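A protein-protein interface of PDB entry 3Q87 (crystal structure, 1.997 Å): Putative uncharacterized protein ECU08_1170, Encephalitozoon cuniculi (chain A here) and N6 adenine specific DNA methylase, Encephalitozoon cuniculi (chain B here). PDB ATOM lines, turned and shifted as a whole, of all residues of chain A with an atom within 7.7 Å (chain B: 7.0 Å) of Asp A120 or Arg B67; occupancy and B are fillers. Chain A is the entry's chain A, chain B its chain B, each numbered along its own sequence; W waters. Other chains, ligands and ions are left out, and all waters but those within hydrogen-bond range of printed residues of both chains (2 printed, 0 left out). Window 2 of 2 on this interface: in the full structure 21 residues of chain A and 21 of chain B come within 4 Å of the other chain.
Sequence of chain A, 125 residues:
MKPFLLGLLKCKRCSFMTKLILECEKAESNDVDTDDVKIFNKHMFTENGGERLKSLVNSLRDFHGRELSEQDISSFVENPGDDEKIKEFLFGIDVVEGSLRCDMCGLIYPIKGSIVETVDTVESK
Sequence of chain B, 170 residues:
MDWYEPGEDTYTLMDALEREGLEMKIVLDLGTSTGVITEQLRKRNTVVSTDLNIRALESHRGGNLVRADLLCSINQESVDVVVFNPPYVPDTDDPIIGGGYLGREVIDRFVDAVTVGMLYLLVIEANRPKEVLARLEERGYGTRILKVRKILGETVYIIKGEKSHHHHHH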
ATOM      1  N   LEU A   9     -12.162  30.057  15.353  1.00  0.00           N
ATOM      2  CA  LEU A   9     -12.146  28.638  15.668  1.00  0.00           C
ATOM      3  C   LEU A   9     -13.473  28.011  15.284  1.00  0.00           C
ATOM      4  O   LEU A   9     -14.486  28.684  15.267  1.00  0.00           O
ATOM      5  CB  LEU A   9     -11.872  28.421  17.152  1.00  0.00           C
ATOM      6  CG  LEU A   9     -10.449  28.611  17.692  1.00  0.00           C
ATOM      7  CD1 LEU A   9     -10.469  28.788  19.195  1.00  0.00           C
ATOM      8  CD2 LEU A   9      -9.577  27.429  17.319  1.00  0.00           C
ATOM      9  N   LYS A  12     -14.332  20.800  14.973  1.00  0.00           N
ATOM     10  CA  LYS A  12     -13.615  20.091  13.927  1.00  0.00           C
ATOM     11  C   LYS A  12     -14.400  18.871  13.445  1.00  0.00           C
ATOM     12  O   LYS A  12     -13.983  18.189  12.510  1.00  0.00           O
ATOM     13  CB  LYS A  12     -12.230  19.682  14.417  1.00  0.00           C
ATOM     14  CG  LYS A  12     -12.256  18.542  15.427  1.00  0.00           C
ATOM     15  CD  LYS A  12     -10.855  18.091  15.776  1.00  0.00           C
ATOM     16  CE  LYS A  12     -10.881  17.078  16.909  1.00  0.00           C
ATOM     17  NZ  LYS A  12      -9.487  16.689  17.275  1.00  0.00           N
ATOM     18  N   LEU A 107     -18.616  18.563  21.548  1.00  0.00           N
ATOM     19  CA  LEU A 107     -17.158  18.424  21.553  1.00  0.00           C
ATOM     20  C   LEU A 107     -16.501  19.549  22.366  1.00  0.00           C
ATOM     21  O   LEU A 107     -16.884  20.717  22.260  1.00  0.00           O
ATOM     22  CB  LEU A 107     -16.618  18.448  20.126  1.00  0.00           C
ATOM     23  CG  LEU A 107     -15.123  18.170  19.957  1.00  0.00           C
ATOM     24  CD1 LEU A 107     -14.863  16.685  20.157  1.00  0.00           C
ATOM     25  CD2 LEU A 107     -14.639  18.609  18.586  1.00  0.00           C
ATOM     26  N   ILE A 108     -15.510  19.186  23.171  1.00  0.00           N
ATOM     27  CA  ILE A 108     -14.830  20.120  24.060  1.00  0.00           C
ATOM     28  C   ILE A 108     -13.361  20.319  23.701  1.00  0.00           C
ATOM     29  O   ILE A 108     -12.610  19.350  23.597  1.00  0.00           O
ATOM     30  CB  ILE A 108     -14.800  19.603  25.503  1.00  0.00           C
ATOM     31  CG1 ILE A 108     -16.210  19.336  26.035  1.00  0.00           C
ATOM     32  CG2 ILE A 108     -14.049  20.572  26.392  1.00  0.00           C
ATOM     33  CD1 ILE A 108     -16.999  20.564  26.248  1.00  0.00           C
ATOM     34  N   TYR A 109     -12.970  21.585  23.547  1.00  0.00           N
ATOM     35  CA  TYR A 109     -11.573  21.984  23.434  1.00  0.00           C
ATOM     36  C   TYR A 109     -11.107  22.571  24.773  1.00  0.00           C
ATOM     37  O   TYR A 109     -11.478  23.679  25.137  1.00  0.00           O
ATOM     38  CB  TYR A 109     -11.396  23.066  22.366  1.00  0.00           C
ATOM     39  CG  TYR A 109     -11.737  22.720  20.925  1.00  0.00           C
ATOM     40  CD1 TYR A 109     -11.678  21.416  20.455  1.00  0.00           C
ATOM     41  CD2 TYR A 109     -12.064  23.726  20.024  1.00  0.00           C
ATOM     42  CE1 TYR A 109     -11.968  21.121  19.140  1.00  0.00           C
ATOM     43  CE2 TYR A 109     -12.358  23.444  18.693  1.00  0.00           C
ATOM     44  CZ  TYR A 109     -12.301  22.148  18.258  1.00  0.00           C
ATOM     45  OH  TYR A 109     -12.578  21.878  16.950  1.00  0.00           O
ATOM     46  N   PRO A 110     -10.277  21.839  25.506  1.00  0.00           N
ATOM     47  CA  PRO A 110      -9.756  22.432  26.740  1.00  0.00           C
ATOM     48  C   PRO A 110      -8.883  23.638  26.412  1.00  0.00           C
ATOM     49  O   PRO A 110      -8.275  23.697  25.349  1.00  0.00           O
ATOM     50  CB  PRO A 110      -8.888  21.313  27.330  1.00  0.00           C
ATOM     51  CG  PRO A 110      -9.369  20.050  26.660  1.00  0.00           C
ATOM     52  CD  PRO A 110      -9.769  20.476  25.283  1.00  0.00           C
ATOM     53  N   ILE A 115      -3.307  28.049  25.937  1.00  0.00           N
ATOM     54  CA  ILE A 115      -3.332  27.382  24.640  1.00  0.00           C
ATOM     55  C   ILE A 115      -4.662  26.663  24.424  1.00  0.00           C
ATOM     56  O   ILE A 115      -5.165  25.999  25.338  1.00  0.00           O
ATOM     57  CB  ILE A 115      -2.208  26.361  24.537  1.00  0.00           C
ATOM     58  CG1 ILE A 115      -0.856  27.064  24.714  1.00  0.00           C
ATOM     59  CG2 ILE A 115      -2.285  25.635  23.194  1.00  0.00           C
ATOM     60  CD1 ILE A 115       0.291  26.113  25.093  1.00  0.00           C
ATOM     61  N   VAL A 116      -5.240  26.809  23.232  1.00  0.00           N
ATOM     62  CA  VAL A 116      -6.453  26.069  22.878  1.00  0.00           C
ATOM     63  C   VAL A 116      -6.093  24.696  22.311  1.00  0.00           C
ATOM     64  O   VAL A 116      -5.361  24.567  21.332  1.00  0.00           O
ATOM     65  CB  VAL A 116      -7.326  26.809  21.864  1.00  0.00           C
ATOM     66  CG1 VAL A 116      -8.612  25.996  21.566  1.00  0.00           C
ATOM     67  CG2 VAL A 116      -7.667  28.221  22.370  1.00  0.00           C
ATOM     68  N   GLU A 117      -6.622  23.672  22.947  1.00  0.00           N
ATOM     69  CA  GLU A 117      -6.247  22.317  22.650  1.00  0.00           C
ATOM     70  C   GLU A 117      -7.332  21.675  21.794  1.00  0.00           C
ATOM     71  O   GLU A 117      -8.392  21.333  22.295  1.00  0.00           O
ATOM     72  CB  GLU A 117      -6.077  21.565  23.966  1.00  0.00           C
ATOM     73  CG  GLU A 117      -6.082  20.068  23.799  1.00  0.00           C
ATOM     74  CD  GLU A 117      -4.823  19.588  23.115  1.00  0.00           C
ATOM     75  OE1 GLU A 117      -3.724  19.770  23.684  1.00  0.00           O
ATOM     76  OE2 GLU A 117      -4.932  19.041  22.002  1.00  0.00           O
ATOM     77  N   THR A 118      -7.081  21.509  20.503  1.00  0.00           N
ATOM     78  CA  THR A 118      -8.124  20.965  19.635  1.00  0.00           C
ATOM     79  C   THR A 118      -7.834  19.543  19.161  1.00  0.00           C
ATOM     80  O   THR A 118      -8.570  18.981  18.347  1.00  0.00           O
ATOM     81  CB  THR A 118      -8.378  21.871  18.408  1.00  0.00           C
ATOM     82  OG1 THR A 118      -7.321  21.708  17.444  1.00  0.00           O
ATOM     83  CG2 THR A 118      -8.509  23.363  18.842  1.00  0.00           C
ATOM     84  N   VAL A 119      -6.751  18.967  19.653  1.00  0.00           N
ATOM     85  CA  VAL A 119      -6.355  17.631  19.226  1.00  0.00           C
ATOM     86  C   VAL A 119      -6.850  16.633  20.253  1.00  0.00           C
ATOM     87  O   VAL A 119      -7.560  15.706  19.912  1.00  0.00           O
ATOM     88  CB  VAL A 119      -4.820  17.493  19.062  1.00  0.00           C
ATOM     89  CG1 VAL A 119      -4.448  16.070  18.607  1.00  0.00           C
ATOM     90  CG2 VAL A 119      -4.298  18.519  18.069  1.00  0.00           C
ATOM     91  N   ASP A 120      -6.483  16.841  21.515  1.00  0.00           N
ATOM     92  CA  ASP A 120      -6.923  15.961  22.593  1.00  0.00           C
ATOM     93  C   ASP A 120      -8.215  16.500  23.199  1.00  0.00           C
ATOM     94  O   ASP A 120      -8.207  17.271  24.159  1.00  0.00           O
ATOM     95  CB  ASP A 120      -5.834  15.806  23.656  1.00  0.00           C
ATOM     96  CG  ASP A 120      -4.576  15.132  23.108  1.00  0.00           C
ATOM     97  OD1 ASP A 120      -4.696  14.284  22.198  1.00  0.00           O
ATOM     98  OD2 ASP A 120      -3.465  15.450  23.590  1.00  0.00           O
ATOM     99  N   THR A 121      -9.326  16.098  22.603  1.00  0.00           N
ATOM    100  CA  THR A 121     -10.621  16.652  22.945  1.00  0.00           C
ATOM    101  C   THR A 121     -11.359  15.829  24.002  1.00  0.00           C
ATOM    102  O   THR A 121     -10.963  14.718  24.337  1.00  0.00           O
ATOM    103  CB  THR A 121     -11.495  16.762  21.705  1.00  0.00           C
ATOM    104  OG1 THR A 121     -11.538  15.491  21.040  1.00  0.00           O
ATOM    105  CG2 THR A 121     -10.927  17.800  20.760  1.00  0.00           C
ATOM    106  N   VAL A 122     -12.445  16.401  24.513  1.00  0.00           N
ATOM    107  CA  VAL A 122     -13.320  15.734  25.463  1.00  0.00           C
ATOM    108  C   VAL A 122     -14.732  15.717  24.879  1.00  0.00           C
ATOM    109  O   VAL A 122     -15.126  16.643  24.182  1.00  0.00           O
ATOM    110  CB  VAL A 122     -13.352  16.501  26.805  1.00  0.00           C
ATOM    111  CG1 VAL A 122     -14.094  15.716  27.851  1.00  0.00           C
ATOM    112  CG2 VAL A 122     -11.945  16.795  27.280  1.00  0.00           C
ATOM    113  N   SER B  49      -1.487  31.395  15.769  1.00  0.00           N
ATOM    114  CA  SER B  49      -0.379  30.471  15.567  1.00  0.00           C
ATOM    115  C   SER B  49      -0.724  29.074  16.064  1.00  0.00           C
ATOM    116  O   SER B  49      -1.170  28.907  17.207  1.00  0.00           O
ATOM    117  CB  SER B  49       0.863  31.010  16.271  1.00  0.00           C
ATOM    118  OG  SER B  49       1.036  32.375  15.944  1.00  0.00           O
ATOM    119  N   THR B  50      -0.542  28.075  15.199  1.00  0.00           N
ATOM    120  CA  THR B  50      -0.957  26.711  15.524  1.00  0.00           C
ATOM    121  C   THR B  50       0.157  25.709  15.299  1.00  0.00           C
ATOM    122  O   THR B  50       1.021  25.920  14.460  1.00  0.00           O
ATOM    123  CB  THR B  50      -2.184  26.245  14.692  1.00  0.00           C
ATOM    124  OG1 THR B  50      -1.762  25.915  13.365  1.00  0.00           O
ATOM    125  CG2 THR B  50      -3.264  27.329  14.636  1.00  0.00           C
ATOM    126  N   ASP B  51       0.137  24.621  16.068  1.00  0.00           N
ATOM    127  CA  ASP B  51       1.094  23.534  15.888  1.00  0.00           C
ATOM    128  C   ASP B  51       0.519  22.262  16.496  1.00  0.00           C
ATOM    129  O   ASP B  51      -0.327  22.308  17.391  1.00  0.00           O
ATOM    130  CB  ASP B  51       2.449  23.862  16.547  1.00  0.00           C
ATOM    131  CG  ASP B  51       3.614  23.156  15.866  1.00  0.00           C
ATOM    132  OD1 ASP B  51       4.432  23.837  15.224  1.00  0.00           O
ATOM    133  OD2 ASP B  51       3.691  21.915  15.943  1.00  0.00           O
ATOM    134  N   LEU B  52       0.947  21.124  15.970  1.00  0.00           N
ATOM    135  CA  LEU B  52       0.588  19.832  16.529  1.00  0.00           C
ATOM    136  C   LEU B  52       1.431  19.559  17.776  1.00  0.00           C
ATOM    137  O   LEU B  52       1.026  18.812  18.663  1.00  0.00           O
ATOM    138  CB  LEU B  52       0.830  18.739  15.482  1.00  0.00           C
ATOM    139  CG  LEU B  52       0.311  17.339  15.792  1.00  0.00           C
ATOM    140  CD1 LEU B  52      -1.209  17.399  15.956  1.00  0.00           C
ATOM    141  CD2 LEU B  52       0.699  16.390  14.658  1.00  0.00           C
ATOM    142  N   ASN B  53       2.605  20.193  17.837  1.00  0.00           N
ATOM    143  CA  ASN B  53       3.606  19.945  18.875  1.00  0.00           C
ATOM    144  C   ASN B  53       3.426  20.817  20.129  1.00  0.00           C
ATOM    145  O   ASN B  53       3.755  22.010  20.125  1.00  0.00           O
ATOM    146  CB  ASN B  53       4.997  20.152  18.258  1.00  0.00           C
ATOM    147  CG  ASN B  53       6.120  19.929  19.234  1.00  0.00           C
ATOM    148  OD1 ASN B  53       5.896  19.630  20.402  1.00  0.00           O
ATOM    149  ND2 ASN B  53       7.349  20.085  18.756  1.00  0.00           N
ATOM    150  N   ILE B  54       2.924  20.221  21.208  1.00  0.00           N
ATOM    151  CA  ILE B  54       2.578  21.011  22.389  1.00  0.00           C
ATOM    152  C   ILE B  54       3.822  21.582  23.084  1.00  0.00           C
ATOM    153  O   ILE B  54       3.803  22.690  23.627  1.00  0.00           O
ATOM    154  CB  ILE B  54       1.712  20.199  23.397  1.00  0.00           C
ATOM    155  CG1 ILE B  54       1.020  21.148  24.371  1.00  0.00           C
ATOM    156  CG2 ILE B  54       2.543  19.155  24.143  1.00  0.00           C
ATOM    157  CD1 ILE B  54       0.058  22.106  23.701  1.00  0.00           C
ATOM    158  N   ARG B  55       4.904  20.818  23.050  1.00  0.00           N
ATOM    159  CA  ARG B  55       6.159  21.265  23.627  1.00  0.00           C
ATOM    160  C   ARG B  55       6.624  22.592  23.024  1.00  0.00           C
ATOM    161  O   ARG B  55       7.084  23.463  23.749  1.00  0.00           O
ATOM    162  CB  ARG B  55       7.232  20.189  23.467  1.00  0.00           C
ATOM    163  CG  ARG B  55       7.414  19.335  24.703  1.00  0.00           C
ATOM    164  CD  ARG B  55       8.208  18.079  24.398  1.00  0.00           C
ATOM    165  NE  ARG B  55       7.317  16.987  24.035  1.00  0.00           N
ATOM    166  CZ  ARG B  55       6.945  16.027  24.872  1.00  0.00           C
ATOM    167  NH1 ARG B  55       7.412  16.020  26.113  1.00  0.00           N
ATOM    168  NH2 ARG B  55       6.116  15.073  24.464  1.00  0.00           N
ATOM    169  N   LEU B  57       4.681  24.841  21.547  1.00  0.00           N
ATOM    170  CA  LEU B  57       3.717  25.849  21.956  1.00  0.00           C
ATOM    171  C   LEU B  57       3.996  26.316  23.380  1.00  0.00           C
ATOM    172  O   LEU B  57       3.807  27.481  23.695  1.00  0.00           O
ATOM    173  CB  LEU B  57       2.277  25.328  21.850  1.00  0.00           C
ATOM    174  CG  LEU B  57       1.707  25.081  20.446  1.00  0.00           C
ATOM    175  CD1 LEU B  57       0.224  24.704  20.552  1.00  0.00           C
ATOM    176  CD2 LEU B  57       1.895  26.285  19.523  1.00  0.00           C
ATOM    177  N   LEU B  65      -2.188  31.060  20.637  1.00  0.00           N
ATOM    178  CA  LEU B  65      -1.746  29.697  20.417  1.00  0.00           C
ATOM    179  C   LEU B  65      -2.892  28.694  20.374  1.00  0.00           C
ATOM    180  O   LEU B  65      -3.757  28.676  21.261  1.00  0.00           O
ATOM    181  CB  LEU B  65      -0.733  29.307  21.495  1.00  0.00           C
ATOM    182  CG  LEU B  65       0.443  30.287  21.639  1.00  0.00           C
ATOM    183  CD1 LEU B  65       1.468  29.734  22.606  1.00  0.00           C
ATOM    184  CD2 LEU B  65       1.102  30.590  20.292  1.00  0.00           C
ATOM    185  N   VAL B  66      -2.884  27.870  19.329  1.00  0.00           N
ATOM    186  CA  VAL B  66      -3.828  26.776  19.183  1.00  0.00           C
ATOM    187  C   VAL B  66      -3.067  25.501  18.882  1.00  0.00           C
ATOM    188  O   VAL B  66      -2.250  25.469  17.960  1.00  0.00           O
ATOM    189  CB  VAL B  66      -4.819  27.049  18.029  1.00  0.00           C
ATOM    190  CG1 VAL B  66      -5.916  25.965  17.991  1.00  0.00           C
ATOM    191  CG2 VAL B  66      -5.432  28.446  18.184  1.00  0.00           C
ATOM    192  N   ARG B  67      -3.291  24.452  19.665  1.00  0.00           N
ATOM    193  CA  ARG B  67      -2.750  23.160  19.264  1.00  0.00           C
ATOM    194  C   ARG B  67      -3.785  22.516  18.346  1.00  0.00           C
ATOM    195  O   ARG B  67      -4.929  22.315  18.747  1.00  0.00           O
ATOM    196  CB  ARG B  67      -2.448  22.258  20.451  1.00  0.00           C
ATOM    197  CG  ARG B  67      -2.120  20.849  19.989  1.00  0.00           C
ATOM    198  CD  ARG B  67      -1.439  20.040  21.037  1.00  0.00           C
ATOM    199  NE  ARG B  67      -0.924  18.784  20.492  1.00  0.00           N
ATOM    200  CZ  ARG B  67      -1.397  17.584  20.809  1.00  0.00           C
ATOM    201  NH1 ARG B  67      -2.404  17.478  21.663  1.00  0.00           N
ATOM    202  NH2 ARG B  67      -0.869  16.494  20.272  1.00  0.00           N
ATOM    203  N   ALA B  68      -3.400  22.243  17.104  1.00  0.00           N
ATOM    204  CA  ALA B  68      -4.352  21.742  16.118  1.00  0.00           C
ATOM    205  C   ALA B  68      -3.659  20.939  15.037  1.00  0.00           C
ATOM    206  O   ALA B  68      -2.468  21.121  14.787  1.00  0.00           O
ATOM    207  CB  ALA B  68      -5.112  22.897  15.487  1.00  0.00           C
ATOM    208  N   ASP B  69      -4.428  20.070  14.383  1.00  0.00           N
ATOM    209  CA  ASP B  69      -3.944  19.269  13.263  1.00  0.00           C
ATOM    210  C   ASP B  69      -4.344  20.001  11.982  1.00  0.00           C
ATOM    211  O   ASP B  69      -5.521  20.041  11.624  1.00  0.00           O
ATOM    212  CB  ASP B  69      -4.561  17.860  13.338  1.00  0.00           C
ATOM    213  CG  ASP B  69      -3.913  16.865  12.375  1.00  0.00           C
ATOM    214  OD1 ASP B  69      -3.251  17.285  11.402  1.00  0.00           O
ATOM    215  OD2 ASP B  69      -4.076  15.655  12.604  1.00  0.00           O
ATOM    216  N   SER B  73      -9.801  22.583  12.883  1.00  0.00           N
ATOM    217  CA  SER B  73     -10.439  23.353  13.942  1.00  0.00           C
ATOM    218  C   SER B  73     -10.398  24.857  13.658  1.00  0.00           C
ATOM    219  O   SER B  73     -10.719  25.680  14.523  1.00  0.00           O
ATOM    220  CB  SER B  73      -9.748  23.061  15.272  1.00  0.00           C
ATOM    221  OG  SER B  73      -8.377  23.419  15.196  1.00  0.00           O
HETATM  222  O   HOH W   1      -2.284  13.933  20.421  1.00  0.00           O
HETATM  223  O   HOH W   2      -7.160  19.603  15.606  1.00  0.00           O
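Of the 14 printed residues of chain B, 7 touch a printed residue of chain A. Printed residues of chain B that touch a printed residue of chain A: Leu B52, Leu B57, Leu B65, Val B66, Arg B67, Ala B68 and Ser B73. Hydrophobic or aromatic side chains of chain B within 4 Å of the printed part of chain A: Leu B52, Leu B57, Leu B65, Val B66 and Ala B68. Of the 14 printed residues of chain A, 8 touch a printed residue of chain B. Printed residues of chain A that touch a printed residue of chain B: Leu A9, Tyr A109, Ile A115, Val A116, Glu A117, Thr A118, Val A119 and Asp A120. Among the printed residues, 18 pairs touch across the chains. Among the printed residues, Asp or Glu carboxylates within 4 Å of a Lys or Arg side-chain nitrogen of the other chain: Glu A117 with Arg B67 (3.0 Å) and Asp A120 with Arg B67 (3.0 Å).
Printed residues of chain B within 4 Å of Ile A115: Leu B57 (3.8 Å), Leu B65 (3.6 Å) and Arg B67 (3.9 Å). Printed residues of chain B within 4 Å of Val A119: Leu B52 (3.9 Å), Arg B67 (3.5 Å) and Ala B68 (3.8 Å). Asp A120 touches one residue of chain B. Ser B49 touches none of the printed residues of chain A. Printed residues of chain A within 4 Å of Arg B67: Ile A115, Val A116, Glu A117, Thr A118, Val A119 and Asp A120. The nearest printed residue of chain B that does not touch Asp A120 is Ile B54 (7.0 Å). The nearest residue of chain A that does not touch Arg B67 is Tyr A109 (7.0 Å). The nearest printed residue of chain B that does not touch Thr A118 is Asp B69 (4.5 Å).
N of Val A116 lies within hydrogen-bond range of O of Leu B65 (3.1 Å). The backbone carbonyl oxygen of Val A116 lies within hydrogen-bond range of the backbone NH of Arg B67 (2.7 Å). The guanidinium group (NH1) of Arg B67 is in salt-bridge range of the side-chain carboxylate (OE2) of Glu A117, at 3.0 Å. The side-chain hydroxyl (OG1) of Thr A118 sits at hydrogen-bond distance from the backbone carbonyl oxygen (O) of Arg B67 (2.8 Å). OG of Ser B73 is in hydrogen-bond range of OG1 of Thr A118, 3.0 Å away. The guanidinium group (NH1) of Arg B67 lies within salt-bridge range of the side-chain carboxylate (OD2) of Asp A120 (3.0 Å).
CD2 of Leu A9 touches CG1 of Val B66, at 3.9997 Å. CA of Leu A9 touches O of Ser B73, 3.5 Å away. Tyr A109 touches Ser B73 (OH to CB, 3.5 Å). Leu B57 touches Ile A115 (CD1 to CG2, 3.8 Å). O of Leu B65 touches CA of Ile A115, at 3.6 Å. N of Arg B67 touches CG2 of Ile A115, at 3.9 Å. Val B66 touches Val A116 (CA to O, 3.4 Å). Val B66 touches Thr A118. OG1 of Thr A118 touches CB of Ala B68, 3.2 Å away. CA of Ala B68 touches CG2 of Val A119, at 3.8 Å.
N of Lys A12 lies within hydrogen-bond range of OH of Tyr A109. O of Thr A118 sits at hydrogen-bond distance from NZ of Lys A12, 2.7 Å away. The backbone carbonyl oxygen (O) of Val A119 lies within hydrogen-bond range of the side-chain amino group (NZ) of Lys A12 (3.4 Å). OE2 of Glu A117 is in hydrogen-bond range of N of Val A119 (3.0 Å). O of Ser B49 lies within hydrogen-bond range of N of Val B66, at 2.9 Å. The backbone NH (N) of Asp B51 lies within hydrogen-bond range of the backbone carbonyl oxygen (O) of Val B66 (3.2 Å).
Water W2 bridges OG1 of Thr A118 (2.8 Å) and N of Asp B69 (3.0 Å). Water W1 bridges the guanidinium group (NH2) of Arg B67 (2.9 Å) and the side-chain carboxylate (OD1) of Asp A120 (3.0 Å).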
